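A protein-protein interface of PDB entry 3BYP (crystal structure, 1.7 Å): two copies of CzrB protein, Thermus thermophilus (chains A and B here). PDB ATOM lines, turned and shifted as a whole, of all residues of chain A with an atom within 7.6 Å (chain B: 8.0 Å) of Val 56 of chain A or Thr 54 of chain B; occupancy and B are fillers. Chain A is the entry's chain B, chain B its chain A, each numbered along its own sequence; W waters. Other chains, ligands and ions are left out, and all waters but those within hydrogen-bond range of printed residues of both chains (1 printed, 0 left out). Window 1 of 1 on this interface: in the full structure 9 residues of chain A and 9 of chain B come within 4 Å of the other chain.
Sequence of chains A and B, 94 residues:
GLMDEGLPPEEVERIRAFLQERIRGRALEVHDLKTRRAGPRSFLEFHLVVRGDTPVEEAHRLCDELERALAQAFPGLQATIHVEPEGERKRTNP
The backbone carbonyl oxygen (O) of Gly 52 of chain B sits at hydrogen-bond distance from the backbone NH (N) of Val 56 of chain A, 3.4 Å away. The backbone carbonyl oxygen (O) of Gly 52 of chain B sits at hydrogen-bond distance from the backbone NH (N) of Glu 57 of chain A (3.0 Å). The backbone carbonyl oxygen (O) of Thr 54 of chain B lies within hydrogen-bond range of the backbone NH (N) of Val 56 of chain A (2.8 Å). N of Val 56 of chain B sits at hydrogen-bond distance from O of Gly 52 of chain A (3.3 Å). The backbone carbonyl oxygen (O) of Thr 54 of chain A lies within hydrogen-bond range of the backbone NH (N) of Val 56 of chain B, at 2.8 Å. The backbone carbonyl oxygen (O) of Gly 52 of chain A is in hydrogen-bond range of the backbone NH (N) of Glu 57 of chain B.
The backbone carbonyl oxygen of Val 50 of chain B is in hydrogen-bond range of the backbone NH of Glu 86 of chain B (2.8 Å). The backbone carbonyl oxygen of Arg 51 of chain B sits at hydrogen-bond distance from the side-chain hydroxyl of Thr 54 of chain B. The side-chain carboxylate (OE2) of Glu 57 of chain A lies within salt-bridge range of the guanidinium group (NE) of Arg 61 of chain A, at 3.8 Å.
Pro 55 of chain B touches Gly 52 of chain A (CB to O, 3.6 Å). O of Thr 54 of chain B touches O of Thr 54 of chain A (3.9 Å). Thr 54 of chain A touches Pro 55 of chain B. Gly 52 of chain B touches Pro 55 of chain A. Thr 54 of chain B touches Pro 55 of chain A (O to CA, 3.5 Å). Pro 85 of chain B touches Val 56 of chain A. Pro 85 of chain B touches Glu 57 of chain A (CB to OE1, 3.3 Å). Glu 57 of chain A touches Glu 86 of chain B (OE1 to O, 3.96 Å). Ala 59 of chain A touches Val 56 of chain B. CB of His 60 of chain A touches CG of Pro 85 of chain B, at 3.9 Å.
Of the printed residues of chain B, Val 56 of chain A touches Gly 52 (3.4 Å), Thr 54 (2.8 Å), Val 83 (3.99 Å) and Pro 85 (3.9 Å). Arg 61 of chain A touches none of the printed residues of chain B. Leu 28 of chain B touches none of the printed residues of chain A. Of the printed residues of chain A, Gly 52 of chain B touches Pro 55, Val 56 and Glu 57. Printed residues of chain A within 4 Å of Thr 54 of chain B: Thr 54, Pro 55 and Val 56. Printed residues of chain A within 4 Å of Pro 55 of chain B: Gly 52 and Thr 54. Printed residues of chain A within 4 Å of Val 56 of chain B: Gly 52, Thr 54 and Ala 59. Printed residues of chain A within 4 Å of Glu 57 of chain B: Gly 52. Printed residues of chain A within 4 Å of Pro 85 of chain B: Val 56, Glu 57 and His 60. The nearest printed residue of chain B that does not touch Val 56 of chain A is Ala 59 of chain B (4.01 Å). The nearest printed residue of chain A that does not touch Glu 86 of chain B is Val 56 of chain A (6.2 Å).
Of the 12 printed residues of chain A, 7 touch a printed residue of chain B. Hydrophobic or aromatic side chains of chain A that line the printed part of chain B: Pro 55, Val 56, Ala 59 and His 60. Of the 22 printed residues of chain B, 8 touch a printed residue of chain A. Printed residues of chain B that touch a printed residue of chain A: Gly 52, Thr 54, Pro 55, Val 56, Glu 57, Val 83, Pro 85 and Glu 86.
Gly 52 of chain A touches Val 56 of chain B, and with the chains exchanged Val 56 of chain A touches Gly 52 of chain B. Gly 52 of chain A touches Glu 57 of chain B, and with the chains exchanged Glu 57 of chain A touches Gly 52 of chain B. Thr 54 of chain A touches its own counterpart, Thr 54 of chain B. Val 56 of chain A touches Val 83 of chain B, but with the chains exchanged Val 83 of chain A does not touch Val 56 of chain B (4.1 Å). 11 positions are printed for both chains. Of the 17 pairs that touch across the chains among the printed residues, 11 have their exchanged pair printed and touching as well.
Water W1 lies within hydrogen-bond range of the backbone carbonyl oxygen (O) of Glu 86 of chain B, the side-chain carboxylate (OE1) of Glu 57 of chain A and the backbone NH (N) of Gly 52 of chain B.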
ATOM      1  N   GLY A  52       4.289  27.317 -18.714  1.00  0.00           N
ATOM      2  CA  GLY A  52       4.761  25.915 -18.709  1.00  0.00           C
ATOM      3  C   GLY A  52       4.568  25.193 -20.022  1.00  0.00           C
ATOM      4  O   GLY A  52       5.399  24.359 -20.406  1.00  0.00           O
ATOM      5  N   ASP A  53       3.487  25.506 -20.736  1.00  0.00           N
ATOM      6  CA  ASP A  53       3.204  24.826 -22.008  1.00  0.00           C
ATOM      7  C   ASP A  53       3.980  25.359 -23.218  1.00  0.00           C
ATOM      8  O   ASP A  53       3.830  24.841 -24.328  1.00  0.00           O
ATOM      9  CB  ASP A  53       1.684  24.728 -22.282  1.00  0.00           C
ATOM     10  CG  ASP A  53       0.997  26.082 -22.338  1.00  0.00           C
ATOM     11  OD1 ASP A  53       1.692  27.102 -22.337  1.00  0.00           O
ATOM     12  OD2 ASP A  53      -0.241  26.110 -22.399  1.00  0.00           O
ATOM     13  N   THR A  54       4.849  26.360 -22.997  1.00  0.00           N
ATOM     14  CA  THR A  54       5.652  26.907 -24.077  1.00  0.00           C
ATOM     15  C   THR A  54       6.536  25.790 -24.649  1.00  0.00           C
ATOM     16  O   THR A  54       7.289  25.173 -23.900  1.00  0.00           O
ATOM     17  CB  THR A  54       6.561  28.046 -23.575  1.00  0.00           C
ATOM     18  OG1 THR A  54       5.759  29.048 -22.927  1.00  0.00           O
ATOM     19  CG2 THR A  54       7.291  28.637 -24.747  1.00  0.00           C
ATOM     20  N   PRO A  55       6.430  25.522 -25.966  1.00  0.00           N
ATOM     21  CA  PRO A  55       7.346  24.556 -26.587  1.00  0.00           C
ATOM     22  C   PRO A  55       8.816  24.947 -26.366  1.00  0.00           C
ATOM     23  O   PRO A  55       9.201  26.124 -26.455  1.00  0.00           O
ATOM     24  CB  PRO A  55       6.987  24.640 -28.075  1.00  0.00           C
ATOM     25  CG  PRO A  55       5.556  25.021 -28.080  1.00  0.00           C
ATOM     26  CD  PRO A  55       5.438  26.038 -26.938  1.00  0.00           C
ATOM     27  N   VAL A  56       9.640  23.946 -26.123  1.00  0.00           N
ATOM     28  CA  VAL A  56      11.078  24.180 -25.987  1.00  0.00           C
ATOM     29  C   VAL A  56      11.669  24.884 -27.237  1.00  0.00           C
ATOM     30  O   VAL A  56      12.497  25.786 -27.101  1.00  0.00           O
ATOM     31  CB  VAL A  56      11.781  22.846 -25.676  1.00  0.00           C
ATOM     32  CG1 VAL A  56      13.294  22.937 -25.918  1.00  0.00           C
ATOM     33  CG2 VAL A  56      11.475  22.418 -24.221  1.00  0.00           C
ATOM     34  N   GLU A  57      11.205  24.525 -28.439  1.00  0.00           N
ATOM     35  CA  GLU A  57      11.656  25.240 -29.661  1.00  0.00           C
ATOM     36  C   GLU A  57      11.351  26.731 -29.587  1.00  0.00           C
ATOM     37  O   GLU A  57      12.179  27.563 -29.957  1.00  0.00           O
ATOM     38  CB  GLU A  57      11.006  24.660 -30.927  1.00  0.00           C
ATOM     39  CG  GLU A  57      11.621  25.259 -32.211  1.00  0.00           C
ATOM     40  CD  GLU A  57      13.154  25.130 -32.221  1.00  0.00           C
ATOM     41  OE1 GLU A  57      13.647  23.995 -32.349  1.00  0.00           O
ATOM     42  OE2 GLU A  57      13.873  26.155 -32.098  1.00  0.00           O
ATOM     43  N   GLU A  58      10.162  27.052 -29.095  1.00  0.00           N
ATOM     44  CA  GLU A  58       9.749  28.463 -29.001  1.00  0.00           C
ATOM     45  C   GLU A  58      10.563  29.225 -27.963  1.00  0.00           C
ATOM     46  O   GLU A  58      10.984  30.348 -28.219  1.00  0.00           O
ATOM     47  CB  GLU A  58       8.250  28.544 -28.702  1.00  0.00           C
ATOM     48  CG  GLU A  58       7.740  29.933 -28.266  1.00  0.00           C
ATOM     49  CD  GLU A  58       8.020  31.104 -29.262  1.00  0.00           C
ATOM     50  OE1 GLU A  58       8.495  30.913 -30.423  1.00  0.00           O
ATOM     51  OE2 GLU A  58       7.762  32.261 -28.854  1.00  0.00           O
ATOM     52  N   ALA A  59      10.791  28.616 -26.800  1.00  0.00           N
ATOM     53  CA  ALA A  59      11.643  29.240 -25.788  1.00  0.00           C
ATOM     54  C   ALA A  59      13.045  29.511 -26.342  1.00  0.00           C
ATOM     55  O   ALA A  59      13.583  30.594 -26.140  1.00  0.00           O
ATOM     56  CB  ALA A  59      11.727  28.359 -24.506  1.00  0.00           C
ATOM     57  N   HIS A  60      13.603  28.540 -27.080  1.00  0.00           N
ATOM     58  CA  HIS A  60      14.922  28.691 -27.697  1.00  0.00           C
ATOM     59  C   HIS A  60      14.964  29.825 -28.713  1.00  0.00           C
ATOM     60  O   HIS A  60      15.882  30.661 -28.693  1.00  0.00           O
ATOM     61  CB  HIS A  60      15.373  27.351 -28.317  1.00  0.00           C
ATOM     62  CG  HIS A  60      16.569  27.473 -29.208  1.00  0.00           C
ATOM     63  ND1 HIS A  60      17.811  27.833 -28.736  1.00  0.00           N
ATOM     64  CD2 HIS A  60      16.706  27.312 -30.545  1.00  0.00           C
ATOM     65  CE1 HIS A  60      18.671  27.866 -29.742  1.00  0.00           C
ATOM     66  NE2 HIS A  60      18.023  27.563 -30.854  1.00  0.00           N
ATOM     67  N   ARG A  61      13.950  29.875 -29.581  1.00  0.00           N
ATOM     68  CA  ARG A  61      13.856  30.920 -30.582  1.00  0.00           C
ATOM     69  C   ARG A  61      13.727  32.287 -29.937  1.00  0.00           C
ATOM     70  O   ARG A  61      14.393  33.228 -30.380  1.00  0.00           O
ATOM     71  CB  ARG A  61      12.703  30.646 -31.544  1.00  0.00           C
ATOM     72  CG  ARG A  61      13.024  29.548 -32.534  1.00  0.00           C
ATOM     73  CD  ARG A  61      11.980  29.504 -33.629  1.00  0.00           C
ATOM     74  NE  ARG A  61      12.315  28.525 -34.666  1.00  0.00           N
ATOM     75  CZ  ARG A  61      11.415  27.724 -35.232  1.00  0.00           C
ATOM     76  NH1 ARG A  61      10.137  27.774 -34.832  1.00  0.00           N
ATOM     77  NH2 ARG A  61      11.787  26.864 -36.170  1.00  0.00           N
ATOM     78  N   LEU A  62      12.923  32.386 -28.872  1.00  0.00           N
ATOM     79  CA  LEU A  62      12.752  33.679 -28.195  1.00  0.00           C
ATOM     80  C   LEU A  62      14.074  34.136 -27.588  1.00  0.00           C
ATOM     81  O   LEU A  62      14.429  35.301 -27.694  1.00  0.00           O
ATOM     82  CB  LEU A  62      11.668  33.578 -27.128  1.00  0.00           C
ATOM     83  CG  LEU A  62      11.453  34.850 -26.304  1.00  0.00           C
ATOM     84  CD1 LEU A  62      11.082  36.035 -27.208  1.00  0.00           C
ATOM     85  CD2 LEU A  62      10.360  34.566 -25.254  1.00  0.00           C
ATOM     86  N   VAL A  83      16.076  30.029 -19.078  1.00  0.00           N
ATOM     87  CA  VAL A  83      14.630  29.831 -19.235  1.00  0.00           C
ATOM     88  C   VAL A  83      14.095  29.034 -18.062  1.00  0.00           C
ATOM     89  O   VAL A  83      14.706  28.041 -17.626  1.00  0.00           O
ATOM     90  CB  VAL A  83      14.287  29.043 -20.532  1.00  0.00           C
ATOM     91  CG1 VAL A  83      12.829  28.643 -20.589  1.00  0.00           C
ATOM     92  CG2 VAL A  83      14.673  29.861 -21.761  1.00  0.00           C
ATOM     93  N   GLY B  25      11.516   7.480 -24.513  1.00  0.00           N
ATOM     94  CA  GLY B  25      10.178   8.029 -24.726  1.00  0.00           C
ATOM     95  C   GLY B  25      10.013   9.464 -24.260  1.00  0.00           C
ATOM     96  O   GLY B  25       8.957  10.059 -24.466  1.00  0.00           O
ATOM     97  N   ARG B  26      11.065  10.038 -23.675  1.00  0.00           N
ATOM     98  CA  ARG B  26      10.971  11.369 -23.057  1.00  0.00           C
ATOM     99  C   ARG B  26      11.997  12.356 -23.592  1.00  0.00           C
ATOM    100  O   ARG B  26      11.823  13.590 -23.475  1.00  0.00           O
ATOM    101  CB  ARG B  26      11.074  11.240 -21.543  1.00  0.00           C
ATOM    102  CG  ARG B  26       9.988  10.338 -20.973  1.00  0.00           C
ATOM    103  CD  ARG B  26      10.116  10.150 -19.484  1.00  0.00           C
ATOM    104  NE  ARG B  26       9.817  11.394 -18.773  1.00  0.00           N
ATOM    105  CZ  ARG B  26       9.969  11.556 -17.462  1.00  0.00           C
ATOM    106  NH1 ARG B  26      10.380  10.532 -16.712  1.00  0.00           N
ATOM    107  NH2 ARG B  26       9.666  12.730 -16.901  1.00  0.00           N
ATOM    108  N   ALA B  27      13.058  11.819 -24.173  1.00  0.00           N
ATOM    109  CA  ALA B  27      14.086  12.643 -24.801  1.00  0.00           C
ATOM    110  C   ALA B  27      14.723  11.826 -25.918  1.00  0.00           C
ATOM    111  O   ALA B  27      14.496  10.608 -26.023  1.00  0.00           O
ATOM    112  CB  ALA B  27      15.114  13.099 -23.777  1.00  0.00           C
ATOM    113  N   LEU B  28      15.476  12.508 -26.774  1.00  0.00           N
ATOM    114  CA  LEU B  28      15.987  11.924 -28.022  1.00  0.00           C
ATOM    115  C   LEU B  28      17.468  11.571 -27.968  1.00  0.00           C
ATOM    116  O   LEU B  28      17.897  10.620 -28.619  1.00  0.00           O
ATOM    117  CB  LEU B  28      15.753  12.876 -29.200  1.00  0.00           C
ATOM    118  CG  LEU B  28      14.319  13.332 -29.482  1.00  0.00           C
ATOM    119  CD1 LEU B  28      14.268  14.343 -30.621  1.00  0.00           C
ATOM    120  CD2 LEU B  28      13.383  12.152 -29.789  1.00  0.00           C
ATOM    121  N   LEU B  48      20.625  17.782 -23.148  1.00  0.00           N
ATOM    122  CA  LEU B  48      19.549  16.820 -23.304  1.00  0.00           C
ATOM    123  C   LEU B  48      18.667  17.281 -24.458  1.00  0.00           C
ATOM    124  O   LEU B  48      18.050  18.346 -24.374  1.00  0.00           O
ATOM    125  CB  LEU B  48      18.747  16.713 -22.003  1.00  0.00           C
ATOM    126  CG  LEU B  48      17.565  15.746 -21.985  1.00  0.00           C
ATOM    127  CD1 LEU B  48      18.024  14.292 -22.155  1.00  0.00           C
ATOM    128  CD2 LEU B  48      16.750  15.911 -20.731  1.00  0.00           C
ATOM    129  N   VAL B  49      18.637  16.504 -25.539  1.00  0.00           N
ATOM    130  CA  VAL B  49      17.867  16.883 -26.724  1.00  0.00           C
ATOM    131  C   VAL B  49      16.450  16.333 -26.599  1.00  0.00           C
ATOM    132  O   VAL B  49      16.270  15.137 -26.360  1.00  0.00           O
ATOM    133  CB  VAL B  49      18.507  16.377 -28.052  1.00  0.00           C
ATOM    134  CG1 VAL B  49      17.715  16.849 -29.254  1.00  0.00           C
ATOM    135  CG2 VAL B  49      19.974  16.814 -28.161  1.00  0.00           C
ATOM    136  N   VAL B  50      15.455  17.207 -26.772  1.00  0.00           N
ATOM    137  CA  VAL B  50      14.045  16.796 -26.735  1.00  0.00           C
ATOM    138  C   VAL B  50      13.343  17.231 -28.025  1.00  0.00           C
ATOM    139  O   VAL B  50      13.829  18.137 -28.728  1.00  0.00           O
ATOM    140  CB  VAL B  50      13.311  17.373 -25.477  1.00  0.00           C
ATOM    141  CG1 VAL B  50      13.906  16.784 -24.171  1.00  0.00           C
ATOM    142  CG2 VAL B  50      13.383  18.899 -25.464  1.00  0.00           C
ATOM    143  N   ARG B  51      12.193  16.629 -28.334  1.00  0.00           N
ATOM    144  CA  ARG B  51      11.360  17.134 -29.429  1.00  0.00           C
ATOM    145  C   ARG B  51      11.100  18.638 -29.265  1.00  0.00           C
ATOM    146  O   ARG B  51      10.891  19.113 -28.140  1.00  0.00           O
ATOM    147  CB  ARG B  51      10.023  16.421 -29.433  1.00  0.00           C
ATOM    148  CG  ARG B  51      10.092  14.959 -29.836  1.00  0.00           C
ATOM    149  CD  ARG B  51       8.708  14.370 -29.698  1.00  0.00           C
ATOM    150  NE  ARG B  51       7.703  15.183 -30.375  1.00  0.00           N
ATOM    151  CZ  ARG B  51       7.309  14.989 -31.632  1.00  0.00           C
ATOM    152  NH1 ARG B  51       7.843  14.009 -32.361  1.00  0.00           N
ATOM    153  NH2 ARG B  51       6.388  15.773 -32.161  1.00  0.00           N
ATOM    154  N   GLY B  52      11.118  19.380 -30.371  1.00  0.00           N
ATOM    155  CA  GLY B  52      10.873  20.836 -30.307  1.00  0.00           C
ATOM    156  C   GLY B  52       9.534  21.196 -29.678  1.00  0.00           C
ATOM    157  O   GLY B  52       9.376  22.263 -29.059  1.00  0.00           O
ATOM    158  N   ASP B  53       8.541  20.326 -29.849  1.00  0.00           N
ATOM    159  CA  ASP B  53       7.234  20.604 -29.267  1.00  0.00           C
ATOM    160  C   ASP B  53       7.083  20.275 -27.768  1.00  0.00           C
ATOM    161  O   ASP B  53       6.010  20.476 -27.186  1.00  0.00           O
ATOM    162  CB  ASP B  53       6.112  19.957 -30.094  1.00  0.00           C
ATOM    163  CG  ASP B  53       6.153  18.449 -30.089  1.00  0.00           C
ATOM    164  OD1 ASP B  53       7.053  17.846 -29.471  1.00  0.00           O
ATOM    165  OD2 ASP B  53       5.248  17.856 -30.730  1.00  0.00           O
ATOM    166  N   THR B  54       8.144  19.772 -27.147  1.00  0.00           N
ATOM    167  CA  THR B  54       8.105  19.416 -25.726  1.00  0.00           C
ATOM    168  C   THR B  54       7.805  20.652 -24.891  1.00  0.00           C
ATOM    169  O   THR B  54       8.509  21.652 -25.009  1.00  0.00           O
ATOM    170  CB  THR B  54       9.468  18.883 -25.266  1.00  0.00           C
ATOM    171  OG1 THR B  54       9.824  17.726 -26.051  1.00  0.00           O
ATOM    172  CG2 THR B  54       9.416  18.490 -23.768  1.00  0.00           C
ATOM    173  N   PRO B  55       6.768  20.608 -24.043  1.00  0.00           N
ATOM    174  CA  PRO B  55       6.576  21.779 -23.162  1.00  0.00           C
ATOM    175  C   PRO B  55       7.765  22.015 -22.224  1.00  0.00           C
ATOM    176  O   PRO B  55       8.382  21.048 -21.738  1.00  0.00           O
ATOM    177  CB  PRO B  55       5.337  21.397 -22.363  1.00  0.00           C
ATOM    178  CG  PRO B  55       4.601  20.418 -23.278  1.00  0.00           C
ATOM    179  CD  PRO B  55       5.712  19.598 -23.857  1.00  0.00           C
ATOM    180  N   VAL B  56       8.083  23.283 -21.970  1.00  0.00           N
ATOM    181  CA  VAL B  56       9.180  23.622 -21.069  1.00  0.00           C
ATOM    182  C   VAL B  56       8.971  22.995 -19.685  1.00  0.00           C
ATOM    183  O   VAL B  56       9.915  22.457 -19.113  1.00  0.00           O
ATOM    184  CB  VAL B  56       9.416  25.169 -20.999  1.00  0.00           C
ATOM    185  CG1 VAL B  56      10.321  25.532 -19.816  1.00  0.00           C
ATOM    186  CG2 VAL B  56      10.051  25.645 -22.299  1.00  0.00           C
ATOM    187  N   GLU B  57       7.739  23.027 -19.171  1.00  0.00           N
ATOM    188  CA  GLU B  57       7.461  22.385 -17.875  1.00  0.00           C
ATOM    189  C   GLU B  57       7.843  20.900 -17.871  1.00  0.00           C
ATOM    190  O   GLU B  57       8.439  20.413 -16.892  1.00  0.00           O
ATOM    191  CB  GLU B  57       5.997  22.544 -17.480  1.00  0.00           C
ATOM    192  CG  GLU B  57       5.606  21.857 -16.159  1.00  0.00           C
ATOM    193  CD  GLU B  57       6.475  22.238 -14.952  1.00  0.00           C
ATOM    194  OE1 GLU B  57       7.076  23.335 -14.921  1.00  0.00           O
ATOM    195  OE2 GLU B  57       6.542  21.429 -14.001  1.00  0.00           O
ATOM    196  N   GLU B  58       7.478  20.197 -18.938  1.00  0.00           N
ATOM    197  CA  GLU B  58       7.781  18.762 -19.080  1.00  0.00           C
ATOM    198  C   GLU B  58       9.286  18.517 -19.098  1.00  0.00           C
ATOM    199  O   GLU B  58       9.801  17.629 -18.395  1.00  0.00           O
ATOM    200  CB  GLU B  58       7.147  18.209 -20.356  1.00  0.00           C
ATOM    201  CG  GLU B  58       7.337  16.706 -20.599  1.00  0.00           C
ATOM    202  CD  GLU B  58       6.687  16.247 -21.912  1.00  0.00           C
ATOM    203  OE1 GLU B  58       5.528  16.629 -22.163  1.00  0.00           O
ATOM    204  OE2 GLU B  58       7.343  15.491 -22.678  1.00  0.00           O
ATOM    205  N   ALA B  59       9.998  19.302 -19.901  1.00  0.00           N
ATOM    206  CA  ALA B  59      11.459  19.195 -19.926  1.00  0.00           C
ATOM    207  C   ALA B  59      12.072  19.470 -18.546  1.00  0.00           C
ATOM    208  O   ALA B  59      13.028  18.792 -18.127  1.00  0.00           O
ATOM    209  CB  ALA B  59      12.034  20.161 -20.953  1.00  0.00           C
ATOM    210  N   HIS B  60      11.545  20.489 -17.864  1.00  0.00           N
ATOM    211  CA  HIS B  60      12.042  20.852 -16.548  1.00  0.00           C
ATOM    212  C   HIS B  60      11.836  19.709 -15.534  1.00  0.00           C
ATOM    213  O   HIS B  60      12.728  19.387 -14.748  1.00  0.00           O
ATOM    214  CB  HIS B  60      11.378  22.138 -16.045  1.00  0.00           C
ATOM    215  CG  HIS B  60      11.741  22.467 -14.632  1.00  0.00           C
ATOM    216  ND1 HIS B  60      10.825  22.443 -13.605  1.00  0.00           N
ATOM    217  CD2 HIS B  60      12.936  22.756 -14.066  1.00  0.00           C
ATOM    218  CE1 HIS B  60      11.429  22.755 -12.471  1.00  0.00           C
ATOM    219  NE2 HIS B  60      12.714  22.941 -12.723  1.00  0.00           N
ATOM    220  N   LEU B  62      11.453  16.511 -16.202  1.00  0.00           N
ATOM    221  CA  LEU B  62      12.387  15.435 -16.544  1.00  0.00           C
ATOM    222  C   LEU B  62      13.773  15.700 -15.956  1.00  0.00           C
ATOM    223  O   LEU B  62      14.383  14.811 -15.337  1.00  0.00           O
ATOM    224  CB  LEU B  62      12.486  15.242 -18.060  1.00  0.00           C
ATOM    225  CG  LEU B  62      13.462  14.194 -18.622  1.00  0.00           C
ATOM    226  CD1 LEU B  62      13.219  12.818 -18.005  1.00  0.00           C
ATOM    227  CD2 LEU B  62      13.320  14.174 -20.155  1.00  0.00           C
ATOM    228  N   VAL B  83      18.751  21.831 -21.654  1.00  0.00           N
ATOM    229  CA  VAL B  83      17.709  21.308 -22.551  1.00  0.00           C
ATOM    230  C   VAL B  83      17.841  22.001 -23.915  1.00  0.00           C
ATOM    231  O   VAL B  83      17.991  23.246 -23.978  1.00  0.00           O
ATOM    232  CB  VAL B  83      16.296  21.521 -21.970  1.00  0.00           C
ATOM    233  CG1 VAL B  83      15.230  21.092 -22.960  1.00  0.00           C
ATOM    234  CG2 VAL B  83      16.139  20.736 -20.649  1.00  0.00           C
ATOM    235  N   GLU B  84      17.786  21.184 -24.971  1.00  0.00           N
ATOM    236  CA  GLU B  84      18.015  21.576 -26.371  1.00  0.00           C
ATOM    237  C   GLU B  84      16.882  21.024 -27.257  1.00  0.00           C
ATOM    238  O   GLU B  84      16.544  19.842 -27.136  1.00  0.00           O
ATOM    239  CB  GLU B  84      19.361  20.978 -26.815  1.00  0.00           C
ATOM    240  CG  GLU B  84      19.794  21.234 -28.261  1.00  0.00           C
ATOM    241  CD  GLU B  84      21.127  20.555 -28.620  1.00  0.00           C
ATOM    242  OE1 GLU B  84      21.770  19.956 -27.739  1.00  0.00           O
ATOM    243  OE2 GLU B  84      21.542  20.625 -29.805  1.00  0.00           O
ATOM    244  N   PRO B  85      16.289  21.853 -28.146  1.00  0.00           N
ATOM    245  CA  PRO B  85      15.276  21.280 -29.032  1.00  0.00           C
ATOM    246  C   PRO B  85      15.947  20.542 -30.196  1.00  0.00           C
ATOM    247  O   PRO B  85      17.057  20.917 -30.607  1.00  0.00           O
ATOM    248  CB  PRO B  85      14.513  22.517 -29.553  1.00  0.00           C
ATOM    249  CG  PRO B  85      15.526  23.606 -29.515  1.00  0.00           C
ATOM    250  CD  PRO B  85      16.485  23.301 -28.394  1.00  0.00           C
ATOM    251  N   GLU B  86      15.282  19.494 -30.690  1.00  0.00           N
ATOM    252  CA  GLU B  86      15.731  18.717 -31.853  1.00  0.00           C
ATOM    253  C   GLU B  86      16.114  19.676 -32.984  1.00  0.00           C
ATOM    254  O   GLU B  86      15.324  20.554 -33.363  1.00  0.00           O
ATOM    255  CB  GLU B  86      14.596  17.800 -32.317  1.00  0.00           C
ATOM    256  CG  GLU B  86      14.976  16.719 -33.356  1.00  0.00           C
ATOM    257  CD  GLU B  86      13.815  15.792 -33.695  1.00  0.00           C
ATOM    258  OE1 GLU B  86      12.650  16.133 -33.396  1.00  0.00           O
ATOM    259  OE2 GLU B  86      14.067  14.708 -34.269  1.00  0.00           O
HETATM  260  O   HOH W   1      12.810  21.198 -32.822  1.00  0.00           O
